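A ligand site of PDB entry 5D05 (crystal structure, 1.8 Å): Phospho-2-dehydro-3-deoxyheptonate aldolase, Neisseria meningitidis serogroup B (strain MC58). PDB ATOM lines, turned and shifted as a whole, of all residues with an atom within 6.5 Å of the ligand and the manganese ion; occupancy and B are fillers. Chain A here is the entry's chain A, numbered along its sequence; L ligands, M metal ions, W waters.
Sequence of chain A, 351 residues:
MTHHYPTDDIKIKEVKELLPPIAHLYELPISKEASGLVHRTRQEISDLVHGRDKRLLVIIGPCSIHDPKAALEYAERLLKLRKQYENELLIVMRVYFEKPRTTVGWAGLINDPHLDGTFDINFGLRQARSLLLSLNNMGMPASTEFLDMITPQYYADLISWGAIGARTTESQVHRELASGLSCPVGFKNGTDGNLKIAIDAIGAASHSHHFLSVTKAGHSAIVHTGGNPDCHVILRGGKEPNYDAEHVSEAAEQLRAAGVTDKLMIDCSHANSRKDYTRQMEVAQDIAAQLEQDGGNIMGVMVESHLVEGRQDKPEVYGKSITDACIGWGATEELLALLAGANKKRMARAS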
ATOM      1  N   PRO A  62       3.739   0.434 -31.292  1.00  0.00           N
ATOM      2  CA  PRO A  62       3.107   0.988 -30.079  1.00  0.00           C
ATOM      3  C   PRO A  62       2.363  -0.022 -29.203  1.00  0.00           C
ATOM      4  O   PRO A  62       1.866  -1.043 -29.700  1.00  0.00           O
ATOM      5  CB  PRO A  62       2.119   1.998 -30.672  1.00  0.00           C
ATOM      6  CG  PRO A  62       2.792   2.459 -31.933  1.00  0.00           C
ATOM      7  CD  PRO A  62       3.366   1.190 -32.496  1.00  0.00           C
ATOM      8  N   CYS A  63       2.289   0.260 -27.897  1.00  0.00           N
ATOM      9  CA  CYS A  63       1.417  -0.518 -27.027  1.00  0.00           C
ATOM     10  C   CYS A  63       0.017  -0.524 -27.612  1.00  0.00           C
ATOM     11  O   CYS A  63      -0.626  -1.597 -27.789  1.00  0.00           O
ATOM     12  CB  CYS A  63       1.386   0.081 -25.618  1.00  0.00           C
ATOM     13  SG  CYS A  63       0.197  -0.741 -24.555  1.00  0.00           S
ATOM     14  N   SER A  64      -0.472   0.663 -27.897  1.00  0.00           N
ATOM     15  CA  SER A  64      -1.755   0.843 -28.564  1.00  0.00           C
ATOM     16  C   SER A  64      -1.688   1.987 -29.579  1.00  0.00           C
ATOM     17  O   SER A  64      -0.887   2.918 -29.447  1.00  0.00           O
ATOM     18  CB  SER A  64      -2.890   1.093 -27.541  1.00  0.00           C
ATOM     19  OG  SER A  64      -2.731   2.301 -26.784  1.00  0.00           O
ATOM     20  N   ARG A  94       3.455  -3.896 -34.791  1.00  0.00           N
ATOM     21  CA  ARG A  94       2.413  -4.107 -33.763  1.00  0.00           C
ATOM     22  C   ARG A  94       1.331  -3.042 -33.952  1.00  0.00           C
ATOM     23  O   ARG A  94       1.579  -1.867 -33.782  1.00  0.00           O
ATOM     24  CB  ARG A  94       3.062  -4.004 -32.398  1.00  0.00           C
ATOM     25  CG  ARG A  94       2.152  -4.173 -31.207  1.00  0.00           C
ATOM     26  CD  ARG A  94       2.882  -4.031 -29.862  1.00  0.00           C
ATOM     27  NE  ARG A  94       1.880  -3.808 -28.821  1.00  0.00           N
ATOM     28  CZ  ARG A  94       1.422  -4.710 -27.937  1.00  0.00           C
ATOM     29  NH1 ARG A  94       1.929  -5.940 -27.841  1.00  0.00           N
ATOM     30  NH2 ARG A  94       0.475  -4.347 -27.099  1.00  0.00           N
ATOM     31  N   TYR A  96      -2.099  -2.740 -32.386  1.00  0.00           N
ATOM     32  CA  TYR A  96      -3.093  -3.126 -31.416  1.00  0.00           C
ATOM     33  C   TYR A  96      -3.920  -1.907 -31.115  1.00  0.00           C
ATOM     34  O   TYR A  96      -3.355  -0.841 -30.879  1.00  0.00           O
ATOM     35  CB  TYR A  96      -2.434  -3.613 -30.151  1.00  0.00           C
ATOM     36  CG  TYR A  96      -1.768  -4.972 -30.180  1.00  0.00           C
ATOM     37  CD1 TYR A  96      -1.129  -5.449 -31.317  1.00  0.00           C
ATOM     38  CD2 TYR A  96      -1.703  -5.748 -29.032  1.00  0.00           C
ATOM     39  CE1 TYR A  96      -0.487  -6.677 -31.315  1.00  0.00           C
ATOM     40  CE2 TYR A  96      -1.047  -6.977 -29.029  1.00  0.00           C
ATOM     41  CZ  TYR A  96      -0.434  -7.429 -30.187  1.00  0.00           C
ATOM     42  OH  TYR A  96       0.239  -8.626 -30.176  1.00  0.00           O
ATOM     43  N   GLU A  98      -6.384  -1.522 -28.654  1.00  0.00           N
ATOM     44  CA  GLU A  98      -6.930  -1.434 -27.325  1.00  0.00           C
ATOM     45  C   GLU A  98      -5.942  -2.136 -26.373  1.00  0.00           C
ATOM     46  O   GLU A  98      -5.268  -3.083 -26.772  1.00  0.00           O
ATOM     47  CB  GLU A  98      -8.251  -2.232 -27.309  1.00  0.00           C
ATOM     48  CG  GLU A  98      -8.944  -2.279 -25.982  1.00  0.00           C
ATOM     49  CD  GLU A  98     -10.317  -2.937 -25.990  1.00  0.00           C
ATOM     50  OE1 GLU A  98     -10.865  -3.265 -27.047  1.00  0.00           O
ATOM     51  OE2 GLU A  98     -10.848  -3.082 -24.900  1.00  0.00           O
ATOM     52  N   LYS A  99      -5.874  -1.697 -25.138  1.00  0.00           N
ATOM     53  CA  LYS A  99      -5.267  -2.528 -24.096  1.00  0.00           C
ATOM     54  C   LYS A  99      -6.396  -2.925 -23.127  1.00  0.00           C
ATOM     55  O   LYS A  99      -7.098  -2.047 -22.622  1.00  0.00           O
ATOM     56  CB  LYS A  99      -4.179  -1.794 -23.295  1.00  0.00           C
ATOM     57  CG  LYS A  99      -3.476  -2.735 -22.330  1.00  0.00           C
ATOM     58  CD  LYS A  99      -2.435  -2.138 -21.372  1.00  0.00           C
ATOM     59  CE  LYS A  99      -1.638  -3.308 -20.780  1.00  0.00           C
ATOM     60  NZ  LYS A  99      -0.923  -2.930 -19.555  1.00  0.00           N
ATOM     61  N   PRO A 100      -6.542  -4.230 -22.855  1.00  0.00           N
ATOM     62  CA  PRO A 100      -7.594  -4.631 -21.898  1.00  0.00           C
ATOM     63  C   PRO A 100      -7.334  -4.038 -20.496  1.00  0.00           C
ATOM     64  O   PRO A 100      -6.162  -3.790 -20.135  1.00  0.00           O
ATOM     65  CB  PRO A 100      -7.489  -6.151 -21.861  1.00  0.00           C
ATOM     66  CG  PRO A 100      -6.779  -6.537 -23.114  1.00  0.00           C
ATOM     67  CD  PRO A 100      -5.839  -5.400 -23.432  1.00  0.00           C
ATOM     68  N   GLU A 145      -3.953  -8.026 -31.799  1.00  0.00           N
ATOM     69  CA  GLU A 145      -4.561  -8.941 -30.850  1.00  0.00           C
ATOM     70  C   GLU A 145      -6.083  -8.975 -31.071  1.00  0.00           C
ATOM     71  O   GLU A 145      -6.728  -7.935 -31.190  1.00  0.00           O
ATOM     72  CB  GLU A 145      -4.264  -8.483 -29.414  1.00  0.00           C
ATOM     73  CG  GLU A 145      -4.731  -9.489 -28.377  1.00  0.00           C
ATOM     74  CD  GLU A 145      -4.029  -9.345 -27.032  1.00  0.00           C
ATOM     75  OE1 GLU A 145      -2.736  -9.493 -26.888  1.00  0.00           O
ATOM     76  OE2 GLU A 145      -4.825  -9.125 -26.117  1.00  0.00           O
ATOM     77  N   ALA A 163      -2.417 -12.252 -32.134  1.00  0.00           N
ATOM     78  CA  ALA A 163      -2.198 -12.663 -30.765  1.00  0.00           C
ATOM     79  C   ALA A 163      -3.489 -12.958 -30.028  1.00  0.00           C
ATOM     80  O   ALA A 163      -4.530 -12.305 -30.252  1.00  0.00           O
ATOM     81  CB  ALA A 163      -1.449 -11.601 -29.992  1.00  0.00           C
ATOM     82  N   ILE A 164      -3.403 -13.900 -29.104  1.00  0.00           N
ATOM     83  CA  ILE A 164      -4.406 -14.086 -28.065  1.00  0.00           C
ATOM     84  C   ILE A 164      -3.724 -13.767 -26.728  1.00  0.00           C
ATOM     85  O   ILE A 164      -2.714 -14.370 -26.372  1.00  0.00           O
ATOM     86  CB  ILE A 164      -4.997 -15.522 -28.069  1.00  0.00           C
ATOM     87  CG1 ILE A 164      -5.734 -15.816 -29.394  1.00  0.00           C
ATOM     88  CG2 ILE A 164      -5.887 -15.705 -26.852  1.00  0.00           C
ATOM     89  CD1 ILE A 164      -6.948 -14.953 -29.688  1.00  0.00           C
ATOM     90  N   GLY A 165      -4.244 -12.763 -26.033  1.00  0.00           N
ATOM     91  CA  GLY A 165      -3.619 -12.280 -24.795  1.00  0.00           C
ATOM     92  C   GLY A 165      -3.737 -13.200 -23.590  1.00  0.00           C
ATOM     93  O   GLY A 165      -4.517 -14.137 -23.568  1.00  0.00           O
ATOM     94  N   ALA A 166      -2.936 -12.900 -22.585  1.00  0.00           N
ATOM     95  CA  ALA A 166      -2.849 -13.670 -21.364  1.00  0.00           C
ATOM     96  C   ALA A 166      -4.184 -13.910 -20.703  1.00  0.00           C
ATOM     97  O   ALA A 166      -4.408 -14.980 -20.147  1.00  0.00           O
ATOM     98  CB  ALA A 166      -1.918 -12.955 -20.386  1.00  0.00           C
ATOM     99  N   LYS A 188      -0.200 -15.863 -25.525  1.00  0.00           N
ATOM    100  CA  LYS A 188       0.626 -15.443 -24.376  1.00  0.00           C
ATOM    101  C   LYS A 188       0.421 -16.377 -23.184  1.00  0.00           C
ATOM    102  O   LYS A 188      -0.679 -16.852 -22.921  1.00  0.00           O
ATOM    103  CB  LYS A 188       0.338 -13.992 -23.976  1.00  0.00           C
ATOM    104  CG  LYS A 188       0.585 -12.978 -25.095  1.00  0.00           C
ATOM    105  CD  LYS A 188       0.758 -11.531 -24.624  1.00  0.00           C
ATOM    106  CE  LYS A 188       2.174 -11.030 -24.834  1.00  0.00           C
ATOM    107  NZ  LYS A 188       2.372  -9.623 -24.380  1.00  0.00           N
ATOM    108  N   ASN A 189       1.491 -16.641 -22.452  1.00  0.00           N
ATOM    109  CA  ASN A 189       1.345 -17.319 -21.174  1.00  0.00           C
ATOM    110  C   ASN A 189       0.490 -16.482 -20.234  1.00  0.00           C
ATOM    111  O   ASN A 189       0.228 -15.296 -20.472  1.00  0.00           O
ATOM    112  CB  ASN A 189       2.731 -17.696 -20.568  1.00  0.00           C
ATOM    113  CG  ASN A 189       3.548 -16.506 -20.058  1.00  0.00           C
ATOM    114  OD1 ASN A 189       4.625 -16.216 -20.600  1.00  0.00           O
ATOM    115  ND2 ASN A 189       3.115 -15.876 -18.971  1.00  0.00           N
ATOM    116  N   ARG A 236       5.873 -13.861 -21.723  1.00  0.00           N
ATOM    117  CA  ARG A 236       5.716 -12.458 -21.319  1.00  0.00           C
ATOM    118  C   ARG A 236       5.835 -12.235 -19.822  1.00  0.00           C
ATOM    119  O   ARG A 236       5.415 -11.225 -19.308  1.00  0.00           O
ATOM    120  CB  ARG A 236       4.399 -11.870 -21.831  1.00  0.00           C
ATOM    121  CG  ARG A 236       3.141 -12.670 -21.566  1.00  0.00           C
ATOM    122  CD  ARG A 236       2.667 -12.646 -20.137  1.00  0.00           C
ATOM    123  NE  ARG A 236       2.170 -11.313 -19.733  1.00  0.00           N
ATOM    124  CZ  ARG A 236       1.982 -10.956 -18.476  1.00  0.00           C
ATOM    125  NH1 ARG A 236       1.524  -9.741 -18.177  1.00  0.00           N
ATOM    126  NH2 ARG A 236       2.283 -11.794 -17.496  1.00  0.00           N
ATOM    127  N   ASP A 267       8.479 -11.812 -25.374  1.00  0.00           N
ATOM    128  CA  ASP A 267       8.096 -10.387 -25.220  1.00  0.00           C
ATOM    129  C   ASP A 267       9.129  -9.721 -24.356  1.00  0.00           C
ATOM    130  O   ASP A 267       9.400 -10.178 -23.230  1.00  0.00           O
ATOM    131  CB  ASP A 267       6.690 -10.315 -24.567  1.00  0.00           C
ATOM    132  CG  ASP A 267       6.085  -8.914 -24.536  1.00  0.00           C
ATOM    133  OD1 ASP A 267       6.746  -7.952 -24.943  1.00  0.00           O
ATOM    134  OD2 ASP A 267       4.902  -8.805 -24.092  1.00  0.00           O
ATOM    135  N   SER A 269       8.729  -6.675 -23.308  1.00  0.00           N
ATOM    136  CA  SER A 269       7.990  -5.656 -22.569  1.00  0.00           C
ATOM    137  C   SER A 269       7.078  -6.325 -21.504  1.00  0.00           C
ATOM    138  O   SER A 269       7.336  -7.474 -21.086  1.00  0.00           O
ATOM    139  CB  SER A 269       7.195  -4.788 -23.544  1.00  0.00           C
ATOM    140  OG  SER A 269       6.773  -3.564 -22.945  1.00  0.00           O
ATOM    141  N   HIS A 270       6.071  -5.597 -21.034  1.00  0.00           N
ATOM    142  CA  HIS A 270       5.087  -6.122 -20.082  1.00  0.00           C
ATOM    143  C   HIS A 270       5.806  -6.732 -18.876  1.00  0.00           C
ATOM    144  O   HIS A 270       6.759  -6.080 -18.372  1.00  0.00           O
ATOM    145  CB  HIS A 270       4.097  -7.027 -20.793  1.00  0.00           C
ATOM    146  CG  HIS A 270       3.402  -6.303 -21.906  1.00  0.00           C
ATOM    147  ND1 HIS A 270       3.626  -6.570 -23.235  1.00  0.00           N
ATOM    148  CD2 HIS A 270       2.568  -5.233 -21.868  1.00  0.00           C
ATOM    149  CE1 HIS A 270       2.915  -5.719 -23.978  1.00  0.00           C
ATOM    150  NE2 HIS A 270       2.273  -4.891 -23.161  1.00  0.00           N
ATOM    151  N   ALA A 271       5.422  -7.918 -18.428  1.00  0.00           N
ATOM    152  CA  ALA A 271       6.012  -8.464 -17.191  1.00  0.00           C
ATOM    153  C   ALA A 271       7.484  -8.915 -17.306  1.00  0.00           C
ATOM    154  O   ALA A 271       8.160  -9.130 -16.287  1.00  0.00           O
ATOM    155  CB  ALA A 271       5.145  -9.583 -16.633  1.00  0.00           C
ATOM    156  N   MET A 302       8.915  -9.643 -29.221  1.00  0.00           N
ATOM    157  CA  MET A 302       7.965  -8.532 -29.239  1.00  0.00           C
ATOM    158  C   MET A 302       8.538  -7.374 -28.456  1.00  0.00           C
ATOM    159  O   MET A 302       9.196  -7.555 -27.417  1.00  0.00           O
ATOM    160  CB  MET A 302       6.609  -9.006 -28.663  1.00  0.00           C
ATOM    161  CG  MET A 302       5.503  -7.963 -28.527  1.00  0.00           C
ATOM    162  SD  MET A 302       3.975  -8.689 -27.839  1.00  0.00           S
ATOM    163  CE  MET A 302       3.414  -9.628 -29.246  1.00  0.00           C
ATOM    164  N   GLU A 304       7.669  -3.071 -27.451  1.00  0.00           N
ATOM    165  CA  GLU A 304       6.807  -1.916 -27.416  1.00  0.00           C
ATOM    166  C   GLU A 304       7.610  -0.647 -27.653  1.00  0.00           C
ATOM    167  O   GLU A 304       8.435  -0.240 -26.824  1.00  0.00           O
ATOM    168  CB  GLU A 304       6.032  -1.856 -26.130  1.00  0.00           C
ATOM    169  CG  GLU A 304       4.974  -2.961 -26.071  1.00  0.00           C
ATOM    170  CD  GLU A 304       4.003  -2.778 -24.918  1.00  0.00           C
ATOM    171  OE1 GLU A 304       4.437  -2.620 -23.742  1.00  0.00           O
ATOM    172  OE2 GLU A 304       2.799  -2.749 -25.177  1.00  0.00           O
ATOM    173  N   THR A 323      -1.049   4.345 -23.290  1.00  0.00           N
ATOM    174  CA  THR A 323      -1.202   3.109 -22.493  1.00  0.00           C
ATOM    175  C   THR A 323       0.186   2.763 -21.923  1.00  0.00           C
ATOM    176  O   THR A 323       0.781   3.612 -21.228  1.00  0.00           O
ATOM    177  CB  THR A 323      -1.920   2.005 -23.305  1.00  0.00           C
ATOM    178  OG1 THR A 323      -1.263   1.804 -24.569  1.00  0.00           O
ATOM    179  CG2 THR A 323      -3.374   2.414 -23.595  1.00  0.00           C
ATOM    180  N   ASP A 324       0.733   1.577 -22.206  1.00  0.00           N
ATOM    181  CA  ASP A 324       2.014   1.221 -21.627  1.00  0.00           C
ATOM    182  C   ASP A 324       3.123   2.099 -22.212  1.00  0.00           C
ATOM    183  O   ASP A 324       3.065   2.490 -23.394  1.00  0.00           O
ATOM    184  CB  ASP A 324       2.379  -0.240 -21.907  1.00  0.00           C
ATOM    185  CG  ASP A 324       1.474  -1.228 -21.175  1.00  0.00           C
ATOM    186  OD1 ASP A 324       0.976  -0.924 -20.090  1.00  0.00           O
ATOM    187  OD2 ASP A 324       1.254  -2.328 -21.692  1.00  0.00           O
ATOM    188  N   ALA A 325       4.135   2.379 -21.391  1.00  0.00           N
ATOM    189  CA  ALA A 325       5.304   3.142 -21.832  1.00  0.00           C
ATOM    190  C   ALA A 325       6.113   2.358 -22.857  1.00  0.00           C
ATOM    191  O   ALA A 325       6.252   1.135 -22.750  1.00  0.00           O
ATOM    192  CB  ALA A 325       6.172   3.553 -20.659  1.00  0.00           C
HETATM  193  C1  LIG L   1       0.696  -8.365 -21.328  1.00  0.00           C
HETATM  194  O1  LIG L   1       1.504  -9.251 -21.703  1.00  0.00           O
HETATM  195  O2  LIG L   1       0.528  -8.107 -20.117  1.00  0.00           O
HETATM  196  C2  LIG L   1      -0.029  -7.585 -22.333  1.00  0.00           C
HETATM  197  C3  LIG L   1      -1.048  -6.765 -22.032  1.00  0.00           C
HETATM  198  O3  LIG L   1       0.522  -7.689 -23.645  1.00  0.00           O
HETATM  199  P1  LIG L   1      -0.277  -7.580 -25.050  1.00  0.00           P
HETATM  200  O4  LIG L   1       0.822  -7.991 -26.005  1.00  0.00           O
HETATM  201  O5  LIG L   1      -1.432  -8.581 -24.966  1.00  0.00           O
HETATM  202  O6  LIG L   1      -0.768  -6.171 -25.157  1.00  0.00           O
HETATM  203 MN    MN M   1       1.311  -2.960 -23.719  1.00  0.00          MN
HETATM  204  O   HOH W   1       0.446  -5.858 -18.899  1.00  0.00           O
HETATM  205  O   HOH W   2      -4.176  -7.906 -20.989  1.00  0.00           O
HETATM  206  O   HOH W   3      -2.102  -9.236 -19.923  1.00  0.00           O
HETATM  207  O   HOH W   4      -3.535  -5.911 -25.584  1.00  0.00           O
HETATM  208  O   HOH W   5      -0.664  -3.835 -24.004  1.00  0.00           O
HETATM  209  O   HOH W   6      -1.843 -10.225 -22.730  1.00  0.00           O
HETATM  210  O   HOH W   7       0.299  -9.926 -27.755  1.00  0.00           O
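NH2 of Arg 94 touches the manganese ion (3.7 Å).
Five residues have an atom within 4 Å of the manganese ion: Cys 63, Arg 94, His 270, Glu 304 and Asp 324.
NH1 of Arg 94 is in hydrogen-bond range of SD of Met 302, 3.4 Å away.
The backbone NH (N) of Ala 271 lies close to the backbone carbonyl oxygen (O) of Arg 236 (3.4 Å).
A ring nitrogen (ND1) of His 270 sits at hydrogen-bond distance from the side-chain amino group (NZ) of Lys 188 (3.5 Å).
O of Ile 164 sits at hydrogen-bond distance from N of Lys 188, 3.0 Å away.
NZ of Lys 99 lies within salt-bridge range of OD1 of Asp 324 (2.8 Å).
The guanidinium group of Arg 94 sits at hydrogen-bond distance from the backbone carbonyl oxygen of Cys 63 (3.0 Å).
N of Arg 236 is in hydrogen-bond range of OD1 of Asn 189 (2.9 Å).
The guanidinium group (NE) of Arg 94 sits at hydrogen-bond distance from the backbone carbonyl oxygen (O) of Pro 62 (2.9 Å).
An oxygen (O4) of the ligand sits close to the side-chain sulfur of Met 302, at 3.7 Å.
Tyr 96 touches the ligand (CE2 to O4, 3.7 Å).
CE of Lys 99 touches C3 of the ligand, at 3.7 Å.
Hydrophobic or aromatic side chains within 4 Å of the ligand: Tyr 96, His 270 and Met 302.
Eight residues have an atom within 4 Å of the ligand: Arg 94, Tyr 96, Lys 99, Glu 145, Lys 188, Arg 236, His 270 and Met 302.
The nearest printed residue that does not touch the ligand is Asp 267 (4.2 Å).
An oxygen (O6) of the ligand is in salt-bridge range of the guanidinium group (NH2) of Arg 94 (2.9 Å).
The side-chain amino group of Lys 188 lies within salt-bridge range of an oxygen (O4) of the ligand (2.8 Å).
An oxygen (O2) of the ligand is in salt-bridge range of the guanidinium group (NH1) of Arg 236 (2.7 Å).
O3 of the ligand sits close to ND1 of His 270, at 3.3 Å.
OE1 of Glu 145 sits close to O5 of the ligand, at 2.5 Å.
Water W5 lies within hydrogen-bond range of O6 of the ligand and NH2 of Arg 94.
Water W1 bridges O2 of the ligand (2.6 Å) and NZ of Lys 99 (3.3 Å).
Water W7 lies within hydrogen-bond range of O4 of the ligand (2.7 Å), OH of Tyr 96 (2.7 Å) and OE1 of Glu 145 (3.2 Å).
Water W6 lies within hydrogen-bond range of an oxygen (O5) of the ligand (2.8 Å) and the backbone NH of Ala 166 (2.9 Å).
The manganese ion is bound by the side-chain carboxylate of Glu 304, the side-chain carboxylate of Asp 324, water W5, a ring nitrogen (NE2) of His 270 and the side-chain sulfur of Cys 63.
The manganese ion has five donor atoms within binding distance.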
